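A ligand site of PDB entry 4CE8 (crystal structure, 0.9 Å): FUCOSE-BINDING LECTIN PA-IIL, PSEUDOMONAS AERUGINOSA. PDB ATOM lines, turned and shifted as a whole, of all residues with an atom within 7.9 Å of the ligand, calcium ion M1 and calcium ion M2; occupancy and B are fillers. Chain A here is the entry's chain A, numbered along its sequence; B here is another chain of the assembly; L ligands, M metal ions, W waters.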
ATOM      1  N   ALA A  20     -10.438 -24.165  17.112  1.00  0.00           N
ATOM      2  CA  ALA A  20     -11.489 -24.843  16.360  1.00  0.00           C
ATOM      3  C   ALA A  20     -12.280 -25.819  17.227  1.00  0.00           C
ATOM      4  O   ALA A  20     -11.722 -26.522  18.077  1.00  0.00           O
ATOM      5  CB  ALA A  20     -10.911 -25.573  15.164  1.00  0.00           C
ATOM      6  N   ASN A  21     -13.591 -25.832  16.982  1.00  0.00           N
ATOM      7  CA  ASN A  21     -14.525 -26.728  17.669  1.00  0.00           C
ATOM      8  C   ASN A  21     -15.655 -27.156  16.737  1.00  0.00           C
ATOM      9  O   ASN A  21     -16.794 -26.699  16.877  1.00  0.00           O
ATOM     10  CB  ASN A  21     -15.146 -26.056  18.911  1.00  0.00           C
ATOM     11  CG  ASN A  21     -14.145 -25.769  19.993  1.00  0.00           C
ATOM     12  OD1 ASN A  21     -13.801 -26.665  20.765  1.00  0.00           O
ATOM     13  ND2 ASN A  21     -13.705 -24.527  20.083  1.00  0.00           N
ATOM     14  N   SER A  22     -15.344 -27.997  15.756  1.00  0.00           N
ATOM     15  CA  SER A  22     -16.316 -28.359  14.719  1.00  0.00           C
ATOM     16  C   SER A  22     -15.810 -29.552  13.946  1.00  0.00           C
ATOM     17  O   SER A  22     -14.593 -29.762  13.827  1.00  0.00           O
ATOM     18  CB  SER A  22     -16.489 -27.204  13.755  1.00  0.00           C
ATOM     19  OG  SER A  22     -17.367 -27.560  12.690  1.00  0.00           O
ATOM     20  N   SER A  23     -16.726 -30.323  13.362  1.00  0.00           N
ATOM     21  CA  SER A  23     -16.317 -31.356  12.404  1.00  0.00           C
ATOM     22  C   SER A  23     -15.741 -30.757  11.115  1.00  0.00           C
ATOM     23  O   SER A  23     -15.004 -31.432  10.401  1.00  0.00           O
ATOM     24  CB  SER A  23     -17.510 -32.259  12.067  1.00  0.00           C
ATOM     25  OG  SER A  23     -18.554 -31.512  11.494  1.00  0.00           O
ATOM     26  N   GLY A  24     -16.078 -29.506  10.810  1.00  0.00           N
ATOM     27  CA  GLY A  24     -15.631 -28.879   9.586  1.00  0.00           C
ATOM     28  C   GLY A  24     -14.294 -28.197   9.727  1.00  0.00           C
ATOM     29  O   GLY A  24     -13.963 -27.619  10.770  1.00  0.00           O
ATOM     30  N   GLN A  26     -11.921 -25.279   9.547  1.00  0.00           N
ATOM     31  CA  GLN A  26     -12.103 -23.831   9.656  1.00  0.00           C
ATOM     32  C   GLN A  26     -11.027 -23.082   8.926  1.00  0.00           C
ATOM     33  O   GLN A  26      -9.864 -23.435   9.017  1.00  0.00           O
ATOM     34  CB  GLN A  26     -12.070 -23.410  11.137  1.00  0.00           C
ATOM     35  CG  GLN A  26     -13.014 -24.196  12.024  1.00  0.00           C
ATOM     36  CD  GLN A  26     -14.456 -23.902  11.674  1.00  0.00           C
ATOM     37  OE1 GLN A  26     -14.871 -22.741  11.607  1.00  0.00           O
ATOM     38  NE2 GLN A  26     -15.234 -24.950  11.471  1.00  0.00           N
ATOM     39  N   GLN A  43      -8.703 -28.234  11.753  1.00  0.00           N
ATOM     40  CA  GLN A  43      -9.894 -28.933  12.166  1.00  0.00           C
ATOM     41  C   GLN A  43      -9.660 -29.552  13.526  1.00  0.00           C
ATOM     42  O   GLN A  43      -8.669 -30.238  13.759  1.00  0.00           O
ATOM     43  CB  GLN A  43     -10.273 -30.008  11.139  1.00  0.00           C
ATOM     44  CG  GLN A  43     -11.637 -30.665  11.436  1.00  0.00           C
ATOM     45  CD  GLN A  43     -11.563 -31.779  12.461  1.00  0.00           C
ATOM     46  OE1 GLN A  43     -10.675 -32.614  12.404  1.00  0.00           O
ATOM     47  NE2 GLN A  43     -12.514 -31.814  13.379  1.00  0.00           N
ATOM     48  N   SER A  44     -10.595 -29.302  14.435  1.00  0.00           N
ATOM     49  CA  SER A  44     -10.554 -29.889  15.768  1.00  0.00           C
ATOM     50  C   SER A  44     -11.952 -29.822  16.359  1.00  0.00           C
ATOM     51  O   SER A  44     -12.671 -28.852  16.111  1.00  0.00           O
ATOM     52  CB  SER A  44      -9.621 -29.061  16.675  1.00  0.00           C
ATOM     53  OG  SER A  44      -9.574 -29.560  18.008  1.00  0.00           O
ATOM     54  N   THR A  45     -12.306 -30.820  17.175  1.00  0.00           N
ATOM     55  CA  THR A  45     -13.462 -30.742  18.055  1.00  0.00           C
ATOM     56  C   THR A  45     -13.058 -30.597  19.514  1.00  0.00           C
ATOM     57  O   THR A  45     -13.889 -30.761  20.418  1.00  0.00           O
ATOM     58  CB  THR A  45     -14.422 -31.922  17.865  1.00  0.00           C
ATOM     59  OG1 THR A  45     -13.682 -33.137  17.885  1.00  0.00           O
ATOM     60  CG2 THR A  45     -15.165 -31.794  16.539  1.00  0.00           C
ATOM     61  N   VAL A  69     -15.989 -22.231   6.082  1.00  0.00           N
ATOM     62  CA  VAL A  69     -15.795 -23.676   6.092  1.00  0.00           C
ATOM     63  C   VAL A  69     -15.990 -24.162   4.653  1.00  0.00           C
ATOM     64  O   VAL A  69     -17.093 -24.092   4.116  1.00  0.00           O
ATOM     65  CB  VAL A  69     -16.749 -24.394   7.062  1.00  0.00           C
ATOM     66  CG1 VAL A  69     -16.623 -25.913   6.922  1.00  0.00           C
ATOM     67  CG2 VAL A  69     -16.455 -23.917   8.489  1.00  0.00           C
ATOM     68  N   SER A  94     -18.034 -17.978  15.841  1.00  0.00           N
ATOM     69  CA  SER A  94     -18.554 -18.220  14.505  1.00  0.00           C
ATOM     70  C   SER A  94     -19.328 -19.523  14.478  1.00  0.00           C
ATOM     71  O   SER A  94     -19.024 -20.465  15.230  1.00  0.00           O
ATOM     72  CB  SER A  94     -17.431 -18.215  13.495  1.00  0.00           C
ATOM     73  OG  SER A  94     -16.526 -19.272  13.667  1.00  0.00           O
ATOM     74  N   GLU A  95     -20.325 -19.559  13.599  1.00  0.00           N
ATOM     75  CA  GLU A  95     -21.242 -20.695  13.478  1.00  0.00           C
ATOM     76  C   GLU A  95     -21.279 -21.167  12.023  1.00  0.00           C
ATOM     77  O   GLU A  95     -21.620 -20.402  11.111  1.00  0.00           O
ATOM     78  CB  GLU A  95     -22.644 -20.318  13.932  1.00  0.00           C
ATOM     79  CG  GLU A  95     -23.644 -21.480  13.818  1.00  0.00           C
ATOM     80  CD  GLU A  95     -23.188 -22.751  14.553  1.00  0.00           C
ATOM     81  OE1 GLU A  95     -22.750 -22.644  15.730  1.00  0.00           O
ATOM     82  OE2 GLU A  95     -23.206 -23.831  13.942  1.00  0.00           O
ATOM     83  N   ASP A  96     -20.925 -22.431  11.834  1.00  0.00           N
ATOM     84  CA  ASP A  96     -20.873 -23.067  10.508  1.00  0.00           C
ATOM     85  C   ASP A  96     -22.052 -24.011  10.223  1.00  0.00           C
ATOM     86  O   ASP A  96     -22.133 -24.552   9.122  1.00  0.00           O
ATOM     87  CB  ASP A  96     -19.529 -23.785  10.352  1.00  0.00           C
ATOM     88  CG  ASP A  96     -19.370 -25.028  11.225  1.00  0.00           C
ATOM     89  OD1 ASP A  96     -20.380 -25.671  11.610  1.00  0.00           O
ATOM     90  OD2 ASP A  96     -18.187 -25.374  11.493  1.00  0.00           O
ATOM     91  N   GLY A  97     -22.954 -24.166  11.186  1.00  0.00           N
ATOM     92  CA  GLY A  97     -23.985 -25.189  11.108  1.00  0.00           C
ATOM     93  C   GLY A  97     -25.291 -24.703  11.669  1.00  0.00           C
ATOM     94  O   GLY A  97     -25.709 -23.578  11.412  1.00  0.00           O
ATOM     95  N   THR A  98     -25.933 -25.573  12.443  1.00  0.00           N
ATOM     96  CA  THR A  98     -27.287 -25.353  12.917  1.00  0.00           C
ATOM     97  C   THR A  98     -27.426 -25.289  14.433  1.00  0.00           C
ATOM     98  O   THR A  98     -28.466 -24.876  14.929  1.00  0.00           O
ATOM     99  CB  THR A  98     -28.223 -26.464  12.404  1.00  0.00           C
ATOM    100  OG1 THR A  98     -27.719 -27.741  12.796  1.00  0.00           O
ATOM    101  CG2 THR A  98     -28.332 -26.417  10.898  1.00  0.00           C
ATOM    102  N   ASP A  99     -26.404 -25.724  15.180  1.00  0.00           N
ATOM    103  CA  ASP A  99     -26.567 -25.828  16.633  1.00  0.00           C
ATOM    104  C   ASP A  99     -26.418 -24.507  17.380  1.00  0.00           C
ATOM    105  O   ASP A  99     -26.805 -24.412  18.534  1.00  0.00           O
ATOM    106  CB  ASP A  99     -25.680 -26.923  17.239  1.00  0.00           C
ATOM    107  CG  ASP A  99     -24.196 -26.643  17.133  1.00  0.00           C
ATOM    108  OD1 ASP A  99     -23.801 -25.656  16.462  1.00  0.00           O
ATOM    109  OD2 ASP A  99     -23.412 -27.436  17.716  1.00  0.00           O
ATOM    110  N   ASN A 100     -25.850 -23.504  16.713  1.00  0.00           N
ATOM    111  CA  ASN A 100     -25.687 -22.175  17.293  1.00  0.00           C
ATOM    112  C   ASN A 100     -24.871 -22.194  18.580  1.00  0.00           C
ATOM    113  O   ASN A 100     -25.111 -21.398  19.489  1.00  0.00           O
ATOM    114  CB  ASN A 100     -27.033 -21.502  17.467  1.00  0.00           C
ATOM    115  CG  ASN A 100     -27.710 -21.263  16.152  1.00  0.00           C
ATOM    116  OD1 ASN A 100     -27.043 -21.157  15.103  1.00  0.00           O
ATOM    117  ND2 ASN A 100     -29.033 -21.197  16.161  1.00  0.00           N
ATOM    118  N   ASP A 101     -23.844 -23.045  18.619  1.00  0.00           N
ATOM    119  CA  ASP A 101     -22.870 -22.923  19.703  1.00  0.00           C
ATOM    120  C   ASP A 101     -21.876 -21.778  19.476  1.00  0.00           C
ATOM    121  O   ASP A 101     -21.264 -21.303  20.424  1.00  0.00           O
ATOM    122  CB  ASP A 101     -22.180 -24.255  20.067  1.00  0.00           C
ATOM    123  CG  ASP A 101     -21.337 -24.904  18.950  1.00  0.00           C
ATOM    124  OD1 ASP A 101     -21.284 -24.366  17.815  1.00  0.00           O
ATOM    125  OD2 ASP A 101     -20.720 -25.956  19.246  1.00  0.00           O
ATOM    126  N   TYR A 102     -21.713 -21.348  18.212  1.00  0.00           N
ATOM    127  CA  TYR A 102     -20.853 -20.199  17.882  1.00  0.00           C
ATOM    128  C   TYR A 102     -19.406 -20.364  18.336  1.00  0.00           C
ATOM    129  O   TYR A 102     -18.698 -19.380  18.446  1.00  0.00           O
ATOM    130  CB  TYR A 102     -21.477 -18.844  18.351  1.00  0.00           C
ATOM    131  CG  TYR A 102     -22.519 -18.385  17.362  1.00  0.00           C
ATOM    132  CD1 TYR A 102     -23.823 -18.866  17.424  1.00  0.00           C
ATOM    133  CD2 TYR A 102     -22.174 -17.542  16.308  1.00  0.00           C
ATOM    134  CE1 TYR A 102     -24.749 -18.511  16.463  1.00  0.00           C
ATOM    135  CE2 TYR A 102     -23.104 -17.175  15.354  1.00  0.00           C
ATOM    136  CZ  TYR A 102     -24.398 -17.665  15.451  1.00  0.00           C
ATOM    137  OH  TYR A 102     -25.352 -17.358  14.498  1.00  0.00           O
ATOM    138  N   ASN A 103     -18.956 -21.610  18.455  1.00  0.00           N
ATOM    139  CA  ASN A 103     -17.572 -21.872  18.846  1.00  0.00           C
ATOM    140  C   ASN A 103     -16.767 -22.548  17.736  1.00  0.00           C
ATOM    141  O   ASN A 103     -15.660 -23.018  17.980  1.00  0.00           O
ATOM    142  CB  ASN A 103     -17.508 -22.727  20.125  1.00  0.00           C
ATOM    143  CG  ASN A 103     -17.908 -24.152  19.856  1.00  0.00           C
ATOM    144  OD1 ASN A 103     -18.277 -24.505  18.730  1.00  0.00           O
ATOM    145  ND2 ASN A 103     -17.857 -24.989  20.878  1.00  0.00           N
ATOM    146  N   ASP A 104     -17.329 -22.605  16.529  1.00  0.00           N
ATOM    147  CA  ASP A 104     -16.783 -23.496  15.513  1.00  0.00           C
ATOM    148  C   ASP A 104     -15.370 -23.078  15.127  1.00  0.00           C
ATOM    149  O   ASP A 104     -14.463 -23.909  15.002  1.00  0.00           O
ATOM    150  CB  ASP A 104     -17.738 -23.593  14.340  1.00  0.00           C
ATOM    151  CG  ASP A 104     -19.105 -24.173  14.753  1.00  0.00           C
ATOM    152  OD1 ASP A 104     -19.157 -25.051  15.663  1.00  0.00           O
ATOM    153  OD2 ASP A 104     -20.127 -23.749  14.201  1.00  0.00           O
ATOM    154  N   ALA A 105     -15.197 -21.758  14.983  1.00  0.00           N
ATOM    155  CA  ALA A 105     -13.896 -21.119  15.132  1.00  0.00           C
ATOM    156  C   ALA A 105     -14.092 -19.988  16.140  1.00  0.00           C
ATOM    157  O   ALA A 105     -15.053 -19.215  16.054  1.00  0.00           O
ATOM    158  CB  ALA A 105     -13.348 -20.564  13.829  1.00  0.00           C
ATOM    159  N   PRO B 112     -18.685 -22.984  25.539  1.00  0.00           N
ATOM    160  CA  PRO B 112     -18.484 -24.427  25.477  1.00  0.00           C
ATOM    161  C   PRO B 112     -17.516 -24.809  24.374  1.00  0.00           C
ATOM    162  O   PRO B 112     -17.209 -24.013  23.465  1.00  0.00           O
ATOM    163  CB  PRO B 112     -19.880 -24.942  25.132  1.00  0.00           C
ATOM    164  CG  PRO B 112     -20.470 -23.885  24.316  1.00  0.00           C
ATOM    165  CD  PRO B 112     -19.953 -22.587  24.901  1.00  0.00           C
ATOM    166  N   LEU B 113     -17.042 -26.050  24.453  1.00  0.00           N
ATOM    167  CA  LEU B 113     -16.158 -26.648  23.449  1.00  0.00           C
ATOM    168  C   LEU B 113     -16.934 -27.650  22.584  1.00  0.00           C
ATOM    169  O   LEU B 113     -18.093 -27.955  22.841  1.00  0.00           O
ATOM    170  CB  LEU B 113     -14.970 -27.341  24.106  1.00  0.00           C
ATOM    171  CG  LEU B 113     -14.129 -26.474  25.037  1.00  0.00           C
ATOM    172  CD1 LEU B 113     -12.882 -27.243  25.420  1.00  0.00           C
ATOM    173  CD2 LEU B 113     -13.755 -25.133  24.393  1.00  0.00           C
ATOM    174  N   GLY B 114     -16.262 -28.148  21.543  1.00  0.00           N
ATOM    175  CA  GLY B 114     -16.816 -29.219  20.739  1.00  0.00           C
ATOM    176  C   GLY B 114     -17.629 -28.811  19.523  1.00  0.00           C
ATOM    177  O   GLY B 114     -18.143 -27.660  19.456  1.00  0.00           O
ATOM    178  OXT GLY B 114     -17.771 -29.682  18.627  1.00  0.00           O
HETATM  179  C1  LIG L   1     -20.438 -28.885  13.432  1.00  0.00           C
HETATM  180  C2  LIG L   1     -20.539 -27.725  14.389  1.00  0.00           C
HETATM  181  C3  LIG L   1     -21.161 -28.206  15.682  1.00  0.00           C
HETATM  182  C4  LIG L   1     -20.306 -29.302  16.329  1.00  0.00           C
HETATM  183  C5  LIG L   1     -20.149 -30.433  15.284  1.00  0.00           C
HETATM  184  C6  LIG L   1     -19.209 -31.524  15.797  1.00  0.00           C
HETATM  185  O1  LIG L   1     -21.737 -29.400  13.131  1.00  0.00           O
HETATM  186  O2  LIG L   1     -21.383 -26.667  13.859  1.00  0.00           O
HETATM  187  O3  LIG L   1     -21.174 -27.065  16.579  1.00  0.00           O
HETATM  188  O4  LIG L   1     -19.032 -28.709  16.614  1.00  0.00           O
HETATM  189  O5  LIG L   1     -19.620 -29.918  14.022  1.00  0.00           O
HETATM  190 CA    CA M   1     -21.765 -24.894  15.559  1.00  0.00          CA
HETATM  191 CA    CA M   2     -19.038 -26.406  17.594  1.00  0.00          CA
HETATM  192  O   HOH W   1     -21.725 -30.476  10.763  1.00  0.00           O
HETATM  193  O   HOH W   2     -23.998 -28.743  10.760  1.00  0.00           O
HETATM  194  O   HOH W   3     -25.018 -30.163  14.059  1.00  0.00           O
HETATM  195  O   HOH W   4     -24.281 -27.567  13.729  1.00  0.00           O
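Water W1 lies within hydrogen-bond range of O1 of the ligand and OG of Ser 23. Water W4 lies within hydrogen-bond range of the backbone NH of Thr 98 (2.9 Å), the backbone NH of Asp 99 (3.2 Å) and an oxygen (O1) of the ligand (3.2 Å).
Calcium ion M2 is bound by OD1 of Asn 103 (2.3 Å), OD1 of Asp 104 (2.4 Å), O of Asn 21 (2.4 Å), OD2 of Asp 101 (2.4 Å), O of Gly 114 of chain B (2.4 Å), O3 of the ligand (2.5 Å) and O4 of the ligand (2.5 Å). Calcium ion M2 has seven donor atoms within binding distance. Slightly farther from calcium ion M2 lies the side-chain carboxylate (OD1) of Asp 101 (3.0 Å).
Of the 25 residues printed, 4 come within 4 Å of calcium ion M1. The nearest printed residue that does not touch calcium ion M1 is Asp 96 (4.3 Å).
O5 of the ligand is in hydrogen-bond range of N of Ser 23 (3.0 Å). The side-chain hydroxyl (OG) of Ser 23 lies within hydrogen-bond range of an oxygen (O5) of the ligand (3.2 Å). The side-chain carboxylate of Asp 96 sits close to an oxygen (O2) of the ligand (2.7 Å).
Ser 22 touches the ligand. N of Gly 97 touches O2 of the ligand, 3.98 Å away. Of the 25 residues printed, 10 come within 4 Å of the ligand. Along chain A the residues within 4 Å of the ligand span positions 21 to 104.
OD1 of Asp 99 binds calcium ion M1 (2.4 Å). Calcium ion M1 is bound by OD1 of Asp 101 (2.4 Å). Calcium ion M1 is bound by OE2 of Glu 95 (2.4 Å). Calcium ion M1 is bound by OD2 of Asp 104, 2.4 Å away. Calcium ion M1 is bound by OE1 of Glu 95 (2.5 Å). Calcium ion M1 is bound by an oxygen (O3) of the ligand (2.5 Å). Calcium ion M1 is bound by an oxygen (O2) of the ligand, 2.5 Å away. The side-chain carboxylate (OD1) of Asp 104 binds calcium ion M1. Calcium ion M1 has eight donor atoms within binding distance.
The side-chain amide nitrogen (ND2) of Asn 103 lies within hydrogen-bond range of the backbone carbonyl oxygen (O) of Pro 112 of chain B. N of Asn 21 lies close to O of Ser 44, 3.3 Å away. OE1 of Glu 95 lies close to N of Asn 100 (3.4 Å). OD2 of Asp 104 lies close to N of Asp 96, 2.8 Å away. The backbone carbonyl oxygen (O) of Ser 22 is in hydrogen-bond range of the side-chain amide nitrogen (NE2) of Gln 43 (3.0 Å). N of Gly 24 is in hydrogen-bond range of OG of Ser 22 (3.0 Å). N of Asp 104 sits at hydrogen-bond distance from O of Ser 94, 3.0 Å away. NE2 of Gln 26 sits at hydrogen-bond distance from OD2 of Asp 96 (3.0 Å).
Within 4 Å of calcium ion M2: Asn 21, Asp 101, Asn 103, Asp 104 and Gly 114 of chain B. Along chain A the residues within 4 Å of calcium ion M2 span positions 21 to 104. The nearest printed residue that does not touch calcium ion M2 is Ser 22 (4.4 Å).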
